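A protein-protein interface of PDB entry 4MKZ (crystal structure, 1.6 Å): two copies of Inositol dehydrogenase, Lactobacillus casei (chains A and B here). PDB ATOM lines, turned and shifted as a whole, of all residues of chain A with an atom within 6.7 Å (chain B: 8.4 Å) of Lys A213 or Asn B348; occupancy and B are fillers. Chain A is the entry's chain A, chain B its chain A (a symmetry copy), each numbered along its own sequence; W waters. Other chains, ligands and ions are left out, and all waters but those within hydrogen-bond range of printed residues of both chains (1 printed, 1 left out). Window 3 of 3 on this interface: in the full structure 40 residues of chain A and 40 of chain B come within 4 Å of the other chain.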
ATOM      1  N   ILE A 211       0.120   8.293   1.870  1.00  0.00           N
ATOM      2  CA  ILE A 211       1.330   9.114   2.051  1.00  0.00           C
ATOM      3  C   ILE A 211       2.525   8.203   2.309  1.00  0.00           C
ATOM      4  O   ILE A 211       2.464   7.327   3.165  1.00  0.00           O
ATOM      5  CB  ILE A 211       1.190  10.090   3.244  1.00  0.00           C
ATOM      6  CG1 ILE A 211      -0.015  11.017   3.041  1.00  0.00           C
ATOM      7  CG2 ILE A 211       2.474  10.924   3.438  1.00  0.00           C
ATOM      8  CD1 ILE A 211      -0.516  11.651   4.326  1.00  0.00           C
ATOM      9  N   ASP A 212       3.619   8.418   1.580  1.00  0.00           N
ATOM     10  CA  ASP A 212       4.761   7.516   1.683  1.00  0.00           C
ATOM     11  C   ASP A 212       5.813   7.982   2.683  1.00  0.00           C
ATOM     12  O   ASP A 212       6.132   7.272   3.630  1.00  0.00           O
ATOM     13  CB  ASP A 212       5.399   7.272   0.322  1.00  0.00           C
ATOM     14  CG  ASP A 212       6.622   6.382   0.412  1.00  0.00           C
ATOM     15  OD1 ASP A 212       6.585   5.376   1.155  1.00  0.00           O
ATOM     16  OD2 ASP A 212       7.628   6.688  -0.250  1.00  0.00           O
ATOM     17  N   LYS A 213       6.365   9.172   2.477  1.00  0.00           N
ATOM     18  CA  LYS A 213       7.335   9.672   3.440  1.00  0.00           C
ATOM     19  C   LYS A 213       7.195  11.174   3.663  1.00  0.00           C
ATOM     20  O   LYS A 213       6.644  11.880   2.820  1.00  0.00           O
ATOM     21  CB  LYS A 213       8.770   9.284   3.052  1.00  0.00           C
ATOM     22  CG  LYS A 213       9.239   9.807   1.696  1.00  0.00           C
ATOM     23  CD  LYS A 213      10.626   9.224   1.342  1.00  0.00           C
ATOM     24  CE  LYS A 213      11.533  10.285   0.725  1.00  0.00           C
ATOM     25  NZ  LYS A 213      12.911   9.762   0.419  1.00  0.00           N
ATOM     26  N   VAL A 214       7.656  11.628   4.825  1.00  0.00           N
ATOM     27  CA  VAL A 214       7.442  13.002   5.261  1.00  0.00           C
ATOM     28  C   VAL A 214       8.689  13.601   5.900  1.00  0.00           C
ATOM     29  O   VAL A 214       9.543  12.893   6.444  1.00  0.00           O
ATOM     30  CB  VAL A 214       6.295  13.101   6.308  1.00  0.00           C
ATOM     31  CG1 VAL A 214       5.013  12.451   5.785  1.00  0.00           C
ATOM     32  CG2 VAL A 214       6.716  12.467   7.635  1.00  0.00           C
ATOM     33  N   TRP A 215       8.798  14.920   5.821  1.00  0.00           N
ATOM     34  CA  TRP A 215       9.750  15.650   6.645  1.00  0.00           C
ATOM     35  C   TRP A 215       8.993  16.817   7.258  1.00  0.00           C
ATOM     36  O   TRP A 215       8.229  17.483   6.573  1.00  0.00           O
ATOM     37  CB  TRP A 215      10.925  16.168   5.802  1.00  0.00           C
ATOM     38  CG  TRP A 215      11.968  16.945   6.594  1.00  0.00           C
ATOM     39  CD1 TRP A 215      12.427  16.674   7.853  1.00  0.00           C
ATOM     40  CD2 TRP A 215      12.676  18.117   6.158  1.00  0.00           C
ATOM     41  NE1 TRP A 215      13.369  17.605   8.228  1.00  0.00           N
ATOM     42  CE2 TRP A 215      13.538  18.502   7.206  1.00  0.00           C
ATOM     43  CE3 TRP A 215      12.661  18.877   4.985  1.00  0.00           C
ATOM     44  CZ2 TRP A 215      14.376  19.613   7.116  1.00  0.00           C
ATOM     45  CZ3 TRP A 215      13.499  19.974   4.893  1.00  0.00           C
ATOM     46  CH2 TRP A 215      14.345  20.335   5.953  1.00  0.00           C
ATOM     47  N   LEU A 238       6.576  18.647   4.373  1.00  0.00           N
ATOM     48  CA  LEU A 238       6.477  18.227   2.987  1.00  0.00           C
ATOM     49  C   LEU A 238       6.247  16.723   2.996  1.00  0.00           C
ATOM     50  O   LEU A 238       6.868  15.997   3.770  1.00  0.00           O
ATOM     51  CB  LEU A 238       7.767  18.567   2.236  1.00  0.00           C
ATOM     52  CG  LEU A 238       7.822  18.230   0.746  1.00  0.00           C
ATOM     53  CD1 LEU A 238       6.728  18.973  -0.027  1.00  0.00           C
ATOM     54  CD2 LEU A 238       9.208  18.579   0.184  1.00  0.00           C
ATOM     55  N   MET A 239       5.326  16.268   2.159  1.00  0.00           N
ATOM     56  CA  MET A 239       4.980  14.855   2.109  1.00  0.00           C
ATOM     57  C   MET A 239       4.945  14.361   0.674  1.00  0.00           C
ATOM     58  O   MET A 239       4.428  15.032  -0.216  1.00  0.00           O
ATOM     59  CB  MET A 239       3.630  14.618   2.794  1.00  0.00           C
ATOM     60  CG  MET A 239       3.511  15.264   4.167  1.00  0.00           C
ATOM     61  SD  MET A 239       2.101  14.698   5.127  1.00  0.00           S
ATOM     62  CE  MET A 239       0.743  15.320   4.153  1.00  0.00           C
ATOM     63  N   GLN A 240       5.482  13.161   0.457  1.00  0.00           N
ATOM     64  CA  GLN A 240       5.467  12.565  -0.864  1.00  0.00           C
ATOM     65  C   GLN A 240       4.480  11.412  -0.829  1.00  0.00           C
ATOM     66  O   GLN A 240       4.590  10.541   0.035  1.00  0.00           O
ATOM     67  CB  GLN A 240       6.855  12.037  -1.217  1.00  0.00           C
ATOM     68  CG  GLN A 240       6.970  11.546  -2.637  1.00  0.00           C
ATOM     69  CD  GLN A 240       8.415  11.377  -3.047  1.00  0.00           C
ATOM     70  OE1 GLN A 240       8.884  12.005  -4.001  1.00  0.00           O
ATOM     71  NE2 GLN A 240       9.138  10.542  -2.312  1.00  0.00           N
ATOM     72  N   LEU A 241       3.516  11.416  -1.748  1.00  0.00           N
ATOM     73  CA  LEU A 241       2.505  10.346  -1.771  1.00  0.00           C
ATOM     74  C   LEU A 241       2.945   9.183  -2.678  1.00  0.00           C
ATOM     75  O   LEU A 241       3.965   9.273  -3.360  1.00  0.00           O
ATOM     76  CB  LEU A 241       1.137  10.889  -2.188  1.00  0.00           C
ATOM     77  CG  LEU A 241       0.291  11.563  -1.102  1.00  0.00           C
ATOM     78  CD1 LEU A 241       0.985  12.767  -0.489  1.00  0.00           C
ATOM     79  CD2 LEU A 241      -1.064  11.964  -1.663  1.00  0.00           C
ATOM     80  N   LYS A 244       3.946   9.711  -6.166  1.00  0.00           N
ATOM     81  CA  LYS A 244       4.818  10.887  -6.193  1.00  0.00           C
ATOM     82  C   LYS A 244       4.019  12.196  -6.237  1.00  0.00           C
ATOM     83  O   LYS A 244       4.561  13.241  -6.604  1.00  0.00           O
ATOM     84  CB  LYS A 244       5.838  10.810  -7.333  1.00  0.00           C
ATOM     85  CG  LYS A 244       6.675   9.534  -7.350  1.00  0.00           C
ATOM     86  CD  LYS A 244       7.955   9.685  -6.545  1.00  0.00           C
ATOM     87  CE  LYS A 244       8.792   8.402  -6.595  1.00  0.00           C
ATOM     88  NZ  LYS A 244       8.024   7.219  -6.113  1.00  0.00           N
ATOM     89  N   ILE A 350      13.786  12.754   7.230  1.00  0.00           N
ATOM     90  CA  ILE A 350      12.675  12.134   6.513  1.00  0.00           C
ATOM     91  C   ILE A 350      12.274  10.825   7.187  1.00  0.00           C
ATOM     92  O   ILE A 350      13.130  10.013   7.560  1.00  0.00           O
ATOM     93  CB  ILE A 350      13.059  11.866   5.048  1.00  0.00           C
ATOM     94  CG1 ILE A 350      13.211  13.196   4.305  1.00  0.00           C
ATOM     95  CG2 ILE A 350      12.038  10.970   4.358  1.00  0.00           C
ATOM     96  CD1 ILE A 350      13.958  13.074   2.997  1.00  0.00           C
ATOM     97  N   VAL A 351      10.971  10.622   7.342  1.00  0.00           N
ATOM     98  CA  VAL A 351      10.452   9.399   7.941  1.00  0.00           C
ATOM     99  C   VAL A 351       9.478   8.729   6.975  1.00  0.00           C
ATOM    100  O   VAL A 351       8.652   9.401   6.362  1.00  0.00           O
ATOM    101  CB  VAL A 351       9.752   9.717   9.262  1.00  0.00           C
ATOM    102  CG1 VAL A 351       9.031   8.484   9.810  1.00  0.00           C
ATOM    103  CG2 VAL A 351      10.751  10.240  10.261  1.00  0.00           C
ATOM    104  N   GLN A 352       9.568   7.405   6.831  1.00  0.00           N
ATOM    105  CA  GLN A 352       8.597   6.672   6.026  1.00  0.00           C
ATOM    106  C   GLN A 352       7.401   6.329   6.908  1.00  0.00           C
ATOM    107  O   GLN A 352       7.576   5.808   8.003  1.00  0.00           O
ATOM    108  CB  GLN A 352       9.214   5.400   5.429  1.00  0.00           C
ATOM    109  CG  GLN A 352      10.329   5.675   4.417  1.00  0.00           C
ATOM    110  CD  GLN A 352      10.205   4.840   3.149  1.00  0.00           C
ATOM    111  OE1 GLN A 352       9.107   4.640   2.630  1.00  0.00           O
ATOM    112  NE2 GLN A 352      11.337   4.344   2.649  1.00  0.00           N
ATOM    113  N   VAL A 353       6.199   6.652   6.443  1.00  0.00           N
ATOM    114  CA  VAL A 353       4.995   6.477   7.246  1.00  0.00           C
ATOM    115  C   VAL A 353       4.769   5.002   7.595  1.00  0.00           C
ATOM    116  O   VAL A 353       4.411   4.674   8.726  1.00  0.00           O
ATOM    117  CB  VAL A 353       3.757   7.051   6.537  1.00  0.00           C
ATOM    118  CG1 VAL A 353       2.483   6.740   7.322  1.00  0.00           C
ATOM    119  CG2 VAL A 353       3.914   8.562   6.345  1.00  0.00           C
ATOM    120  N   ALA A 354       5.019   4.122   6.632  1.00  0.00           N
ATOM    121  CA  ALA A 354       4.745   2.690   6.816  1.00  0.00           C
ATOM    122  C   ALA A 354       5.678   2.019   7.825  1.00  0.00           C
ATOM    123  O   ALA A 354       5.437   0.883   8.236  1.00  0.00           O
ATOM    124  CB  ALA A 354       4.804   1.965   5.477  1.00  0.00           C
ATOM    125  N   VAL B 214      17.556  21.560   2.941  1.00  0.00           N
ATOM    126  CA  VAL B 214      16.379  21.492   2.084  1.00  0.00           C
ATOM    127  C   VAL B 214      16.022  20.058   1.715  1.00  0.00           C
ATOM    128  O   VAL B 214      16.873  19.163   1.687  1.00  0.00           O
ATOM    129  CB  VAL B 214      16.591  22.272   0.755  1.00  0.00           C
ATOM    130  CG1 VAL B 214      17.032  23.712   1.023  1.00  0.00           C
ATOM    131  CG2 VAL B 214      17.607  21.556  -0.138  1.00  0.00           C
ATOM    132  N   TRP B 215      14.743  19.837   1.439  1.00  0.00           N
ATOM    133  CA  TRP B 215      14.313  18.617   0.774  1.00  0.00           C
ATOM    134  C   TRP B 215      13.381  19.037  -0.351  1.00  0.00           C
ATOM    135  O   TRP B 215      12.527  19.891  -0.155  1.00  0.00           O
ATOM    136  CB  TRP B 215      13.578  17.686   1.750  1.00  0.00           C
ATOM    137  CG  TRP B 215      13.094  16.383   1.128  1.00  0.00           C
ATOM    138  CD1 TRP B 215      13.744  15.612   0.204  1.00  0.00           C
ATOM    139  CD2 TRP B 215      11.854  15.711   1.402  1.00  0.00           C
ATOM    140  NE1 TRP B 215      12.986  14.509  -0.116  1.00  0.00           N
ATOM    141  CE2 TRP B 215      11.821  14.548   0.605  1.00  0.00           C
ATOM    142  CE3 TRP B 215      10.772  15.982   2.243  1.00  0.00           C
ATOM    143  CZ2 TRP B 215      10.747  13.659   0.623  1.00  0.00           C
ATOM    144  CZ3 TRP B 215       9.710  15.095   2.267  1.00  0.00           C
ATOM    145  CH2 TRP B 215       9.703  13.947   1.461  1.00  0.00           C
ATOM    146  N   ALA B 216      13.557  18.456  -1.530  1.00  0.00           N
ATOM    147  CA  ALA B 216      12.714  18.799  -2.669  1.00  0.00           C
ATOM    148  C   ALA B 216      12.194  17.525  -3.312  1.00  0.00           C
ATOM    149  O   ALA B 216      12.909  16.524  -3.408  1.00  0.00           O
ATOM    150  CB  ALA B 216      13.474  19.633  -3.678  1.00  0.00           C
ATOM    151  N   ILE B 217      10.945  17.568  -3.747  1.00  0.00           N
ATOM    152  CA  ILE B 217      10.352  16.469  -4.492  1.00  0.00           C
ATOM    153  C   ILE B 217       9.692  17.021  -5.748  1.00  0.00           C
ATOM    154  O   ILE B 217       9.507  18.232  -5.898  1.00  0.00           O
ATOM    155  CB  ILE B 217       9.330  15.682  -3.653  1.00  0.00           C
ATOM    156  CG1 ILE B 217       8.151  16.571  -3.245  1.00  0.00           C
ATOM    157  CG2 ILE B 217      10.005  15.086  -2.421  1.00  0.00           C
ATOM    158  CD1 ILE B 217       7.157  15.870  -2.303  1.00  0.00           C
ATOM    159  N   GLY B 218       9.342  16.136  -6.664  1.00  0.00           N
ATOM    160  CA  GLY B 218       8.779  16.598  -7.909  1.00  0.00           C
ATOM    161  C   GLY B 218       8.112  15.492  -8.670  1.00  0.00           C
ATOM    162  O   GLY B 218       8.237  14.309  -8.337  1.00  0.00           O
ATOM    163  N   LEU B 341      18.643  22.292  -3.826  1.00  0.00           N
ATOM    164  CA  LEU B 341      17.296  21.802  -4.109  1.00  0.00           C
ATOM    165  C   LEU B 341      17.336  20.734  -5.189  1.00  0.00           C
ATOM    166  O   LEU B 341      16.644  19.724  -5.106  1.00  0.00           O
ATOM    167  CB  LEU B 341      16.388  22.953  -4.549  1.00  0.00           C
ATOM    168  CG  LEU B 341      16.072  23.989  -3.476  1.00  0.00           C
ATOM    169  CD1 LEU B 341      15.492  25.233  -4.123  1.00  0.00           C
ATOM    170  CD2 LEU B 341      15.064  23.433  -2.477  1.00  0.00           C
ATOM    171  N   GLN B 342      18.168  20.953  -6.197  1.00  0.00           N
ATOM    172  CA  GLN B 342      18.318  20.004  -7.287  1.00  0.00           C
ATOM    173  C   GLN B 342      18.881  18.680  -6.786  1.00  0.00           C
ATOM    174  O   GLN B 342      18.421  17.597  -7.166  1.00  0.00           O
ATOM    175  CB  GLN B 342      19.277  20.578  -8.319  1.00  0.00           C
ATOM    176  CG  GLN B 342      18.912  20.222  -9.720  1.00  0.00           C
ATOM    177  CD  GLN B 342      17.559  20.774 -10.103  1.00  0.00           C
ATOM    178  OE1 GLN B 342      17.356  21.991 -10.143  1.00  0.00           O
ATOM    179  NE2 GLN B 342      16.620  19.883 -10.374  1.00  0.00           N
ATOM    180  N   GLU B 343      19.890  18.782  -5.933  1.00  0.00           N
ATOM    181  CA  GLU B 343      20.554  17.606  -5.397  1.00  0.00           C
ATOM    182  C   GLU B 343      19.594  16.846  -4.490  1.00  0.00           C
ATOM    183  O   GLU B 343      19.517  15.616  -4.542  1.00  0.00           O
ATOM    184  CB  GLU B 343      21.811  18.013  -4.633  1.00  0.00           C
ATOM    185  CG  GLU B 343      22.601  16.826  -4.106  1.00  0.00           C
ATOM    186  CD  GLU B 343      23.804  17.239  -3.294  1.00  0.00           C
ATOM    187  OE1 GLU B 343      24.213  18.419  -3.393  1.00  0.00           O
ATOM    188  OE2 GLU B 343      24.335  16.380  -2.552  1.00  0.00           O
ATOM    189  N   ALA B 344      18.858  17.588  -3.671  1.00  0.00           N
ATOM    190  CA  ALA B 344      17.861  16.986  -2.784  1.00  0.00           C
ATOM    191  C   ALA B 344      16.791  16.267  -3.576  1.00  0.00           C
ATOM    192  O   ALA B 344      16.316  15.217  -3.163  1.00  0.00           O
ATOM    193  CB  ALA B 344      17.239  18.027  -1.894  1.00  0.00           C
ATOM    194  N   PHE B 345      16.394  16.838  -4.704  1.00  0.00           N
ATOM    195  CA  PHE B 345      15.425  16.174  -5.558  1.00  0.00           C
ATOM    196  C   PHE B 345      15.980  14.877  -6.158  1.00  0.00           C
ATOM    197  O   PHE B 345      15.325  13.836  -6.127  1.00  0.00           O
ATOM    198  CB  PHE B 345      14.945  17.097  -6.682  1.00  0.00           C
ATOM    199  CG  PHE B 345      14.253  16.356  -7.779  1.00  0.00           C
ATOM    200  CD1 PHE B 345      12.980  15.847  -7.580  1.00  0.00           C
ATOM    201  CD2 PHE B 345      14.886  16.124  -8.988  1.00  0.00           C
ATOM    202  CE1 PHE B 345      12.346  15.128  -8.576  1.00  0.00           C
ATOM    203  CE2 PHE B 345      14.257  15.409  -9.986  1.00  0.00           C
ATOM    204  CZ  PHE B 345      12.988  14.916  -9.781  1.00  0.00           C
ATOM    205  N   GLU B 346      17.186  14.940  -6.710  1.00  0.00           N
ATOM    206  CA  GLU B 346      17.785  13.762  -7.337  1.00  0.00           C
ATOM    207  C   GLU B 346      18.046  12.623  -6.349  1.00  0.00           C
ATOM    208  O   GLU B 346      17.832  11.461  -6.669  1.00  0.00           O
ATOM    209  CB  GLU B 346      19.067  14.146  -8.082  1.00  0.00           C
ATOM    210  CG  GLU B 346      18.808  15.031  -9.289  1.00  0.00           C
ATOM    211  CD  GLU B 346      20.071  15.652  -9.843  1.00  0.00           C
ATOM    212  OE1 GLU B 346      21.141  15.493  -9.216  1.00  0.00           O
ATOM    213  OE2 GLU B 346      19.989  16.313 -10.902  1.00  0.00           O
ATOM    214  N   LYS B 347      18.498  12.960  -5.147  1.00  0.00           N
ATOM    215  CA  LYS B 347      18.766  11.953  -4.125  1.00  0.00           C
ATOM    216  C   LYS B 347      17.502  11.538  -3.385  1.00  0.00           C
ATOM    217  O   LYS B 347      17.483  10.503  -2.707  1.00  0.00           O
ATOM    218  CB  LYS B 347      19.783  12.486  -3.114  1.00  0.00           C
ATOM    219  CG  LYS B 347      21.183  12.674  -3.684  1.00  0.00           C
ATOM    220  CD  LYS B 347      22.162  13.127  -2.609  1.00  0.00           C
ATOM    221  CE  LYS B 347      23.588  12.738  -2.978  1.00  0.00           C
ATOM    222  NZ  LYS B 347      23.944  13.197  -4.344  1.00  0.00           N
ATOM    223  N   ASN B 348      16.447  12.338  -3.534  1.00  0.00           N
ATOM    224  CA  ASN B 348      15.256  12.256  -2.677  1.00  0.00           C
ATOM    225  C   ASN B 348      15.639  12.166  -1.193  1.00  0.00           C
ATOM    226  O   ASN B 348      15.265  11.223  -0.494  1.00  0.00           O
ATOM    227  CB  ASN B 348      14.320  11.107  -3.091  1.00  0.00           C
ATOM    228  CG  ASN B 348      12.907  11.277  -2.545  1.00  0.00           C
ATOM    229  OD1 ASN B 348      12.661  12.098  -1.659  1.00  0.00           O
ATOM    230  ND2 ASN B 348      11.977  10.482  -3.063  1.00  0.00           N
ATOM    231  N   ASP B 349      16.392  13.154  -0.725  1.00  0.00           N
ATOM    232  CA  ASP B 349      16.854  13.205   0.656  1.00  0.00           C
ATOM    233  C   ASP B 349      17.156  14.653   1.021  1.00  0.00           C
ATOM    234  O   ASP B 349      17.247  15.521   0.144  1.00  0.00           O
ATOM    235  CB  ASP B 349      18.122  12.352   0.807  1.00  0.00           C
ATOM    236  CG  ASP B 349      18.322  11.829   2.222  1.00  0.00           C
ATOM    237  OD1 ASP B 349      17.616  12.264   3.158  1.00  0.00           O
ATOM    238  OD2 ASP B 349      19.211  10.967   2.401  1.00  0.00           O
ATOM    239  N   ILE B 350      17.303  14.914   2.315  1.00  0.00           N
ATOM    240  CA  ILE B 350      17.658  16.243   2.803  1.00  0.00           C
ATOM    241  C   ILE B 350      19.106  16.569   2.445  1.00  0.00           C
ATOM    242  O   ILE B 350      20.004  15.733   2.603  1.00  0.00           O
ATOM    243  CB  ILE B 350      17.469  16.329   4.327  1.00  0.00           C
ATOM    244  CG1 ILE B 350      15.977  16.257   4.664  1.00  0.00           C
ATOM    245  CG2 ILE B 350      18.097  17.594   4.898  1.00  0.00           C
ATOM    246  CD1 ILE B 350      15.703  15.935   6.116  1.00  0.00           C
ATOM    247  N   VAL B 351      19.328  17.786   1.964  1.00  0.00           N
ATOM    248  CA  VAL B 351      20.669  18.238   1.614  1.00  0.00           C
ATOM    249  C   VAL B 351      20.999  19.514   2.385  1.00  0.00           C
ATOM    250  O   VAL B 351      20.160  20.405   2.493  1.00  0.00           O
ATOM    251  CB  VAL B 351      20.763  18.489   0.108  1.00  0.00           C
ATOM    252  CG1 VAL B 351      22.094  19.149  -0.255  1.00  0.00           C
ATOM    253  CG2 VAL B 351      20.585  17.196  -0.642  1.00  0.00           C
HETATM  254  O   HOH W   1      10.557  13.347  -6.009  1.00  0.00           O
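No residue of chain B comes within 4 Å of Asp A212.
Lys A213 touches just these residues of chain B: Trp B215 (3.5 Å) and Asn B348 (2.9 Å).
No residue of chain B comes within 4 Å of Val A214.
Of the printed residues of chain B, Leu A238 touches Trp B215 (3.3 Å) and Ile B217 (3.9 Å).
Of the printed residues of chain B, Met A239 touches Ile B217 (3.5 Å).
Glu B346 touches none of the printed residues of chain A.
Asn B348 touches just these residues of chain A: Lys A213 (2.9 Å) and Gln A240 (2.9 Å).
The nearest residue of chain B that does not touch Lys A213 is Asp B349 (5.0 Å).
Trp B215 touches its own counterpart, Trp A215.
Trp A215 touches Ile B350, and with the chains exchanged Ile A350 touches Trp B215.
Ile B350 touches its own counterpart, Ile A350.
4 positions are printed for both chains.
Of the 12 pairs that touch across the chains among the printed residues, 4 have their exchanged pair printed and touching as well.
Among the printed residues, pairs that only touch across the chains: Lys A213 with Trp B215 (3.5 Å), Trp A215 with Trp B215 (3.6 Å), Trp A215 with Ile B350 (3.5 Å), Leu A238 with Trp B215 (3.3 Å), Leu A238 with Ile B217 (3.9 Å), Met A239 with Ile B217 (3.5 Å), Gln A240 with Ile B217 (3.6 Å), Ile A350 with Trp B215 (3.5 Å), Ile A350 with Asp B349 (3.7 Å) and Ile A350 with Ile B350 (3.9 Å).
O of Asn B348 is in hydrogen-bond range of NZ of Lys A213, 2.9 Å away.
ND2 of Asn B348 sits close to NE2 of Gln A240 (2.9 Å).
Printed residues of chain B that touch a printed residue of chain A: Trp B215, Ile B217, Asn B348, Asp B349 and Ile B350.
Of the 15 printed residues of chain A, 6 touch a printed residue of chain B.
Among the printed residues, 12 pairs touch across the chains.
Among the printed residues, no Asp or Glu carboxylate lies within 4 Å of a Lys or Arg side-chain nitrogen of the other chain.
Water W1 bridges OE1 of Gln A240 (2.9 Å) and N of Gly B218 (3.1 Å).
The backbone carbonyl oxygen (O) of Gln A240 lies within hydrogen-bond range of the backbone NH (N) of Asp A212, at 2.8 Å.
O of Lys A213 sits at hydrogen-bond distance from N of Gln A240.
O of Trp A215 is in hydrogen-bond range of N of Leu A238 (3.0 Å).
The side-chain amide oxygen of Asn B348 is in hydrogen-bond range of the indole nitrogen of Trp B215.
The backbone NH of Asp B349 lies within hydrogen-bond range of the backbone carbonyl oxygen of Ala B344 (3.2 Å).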
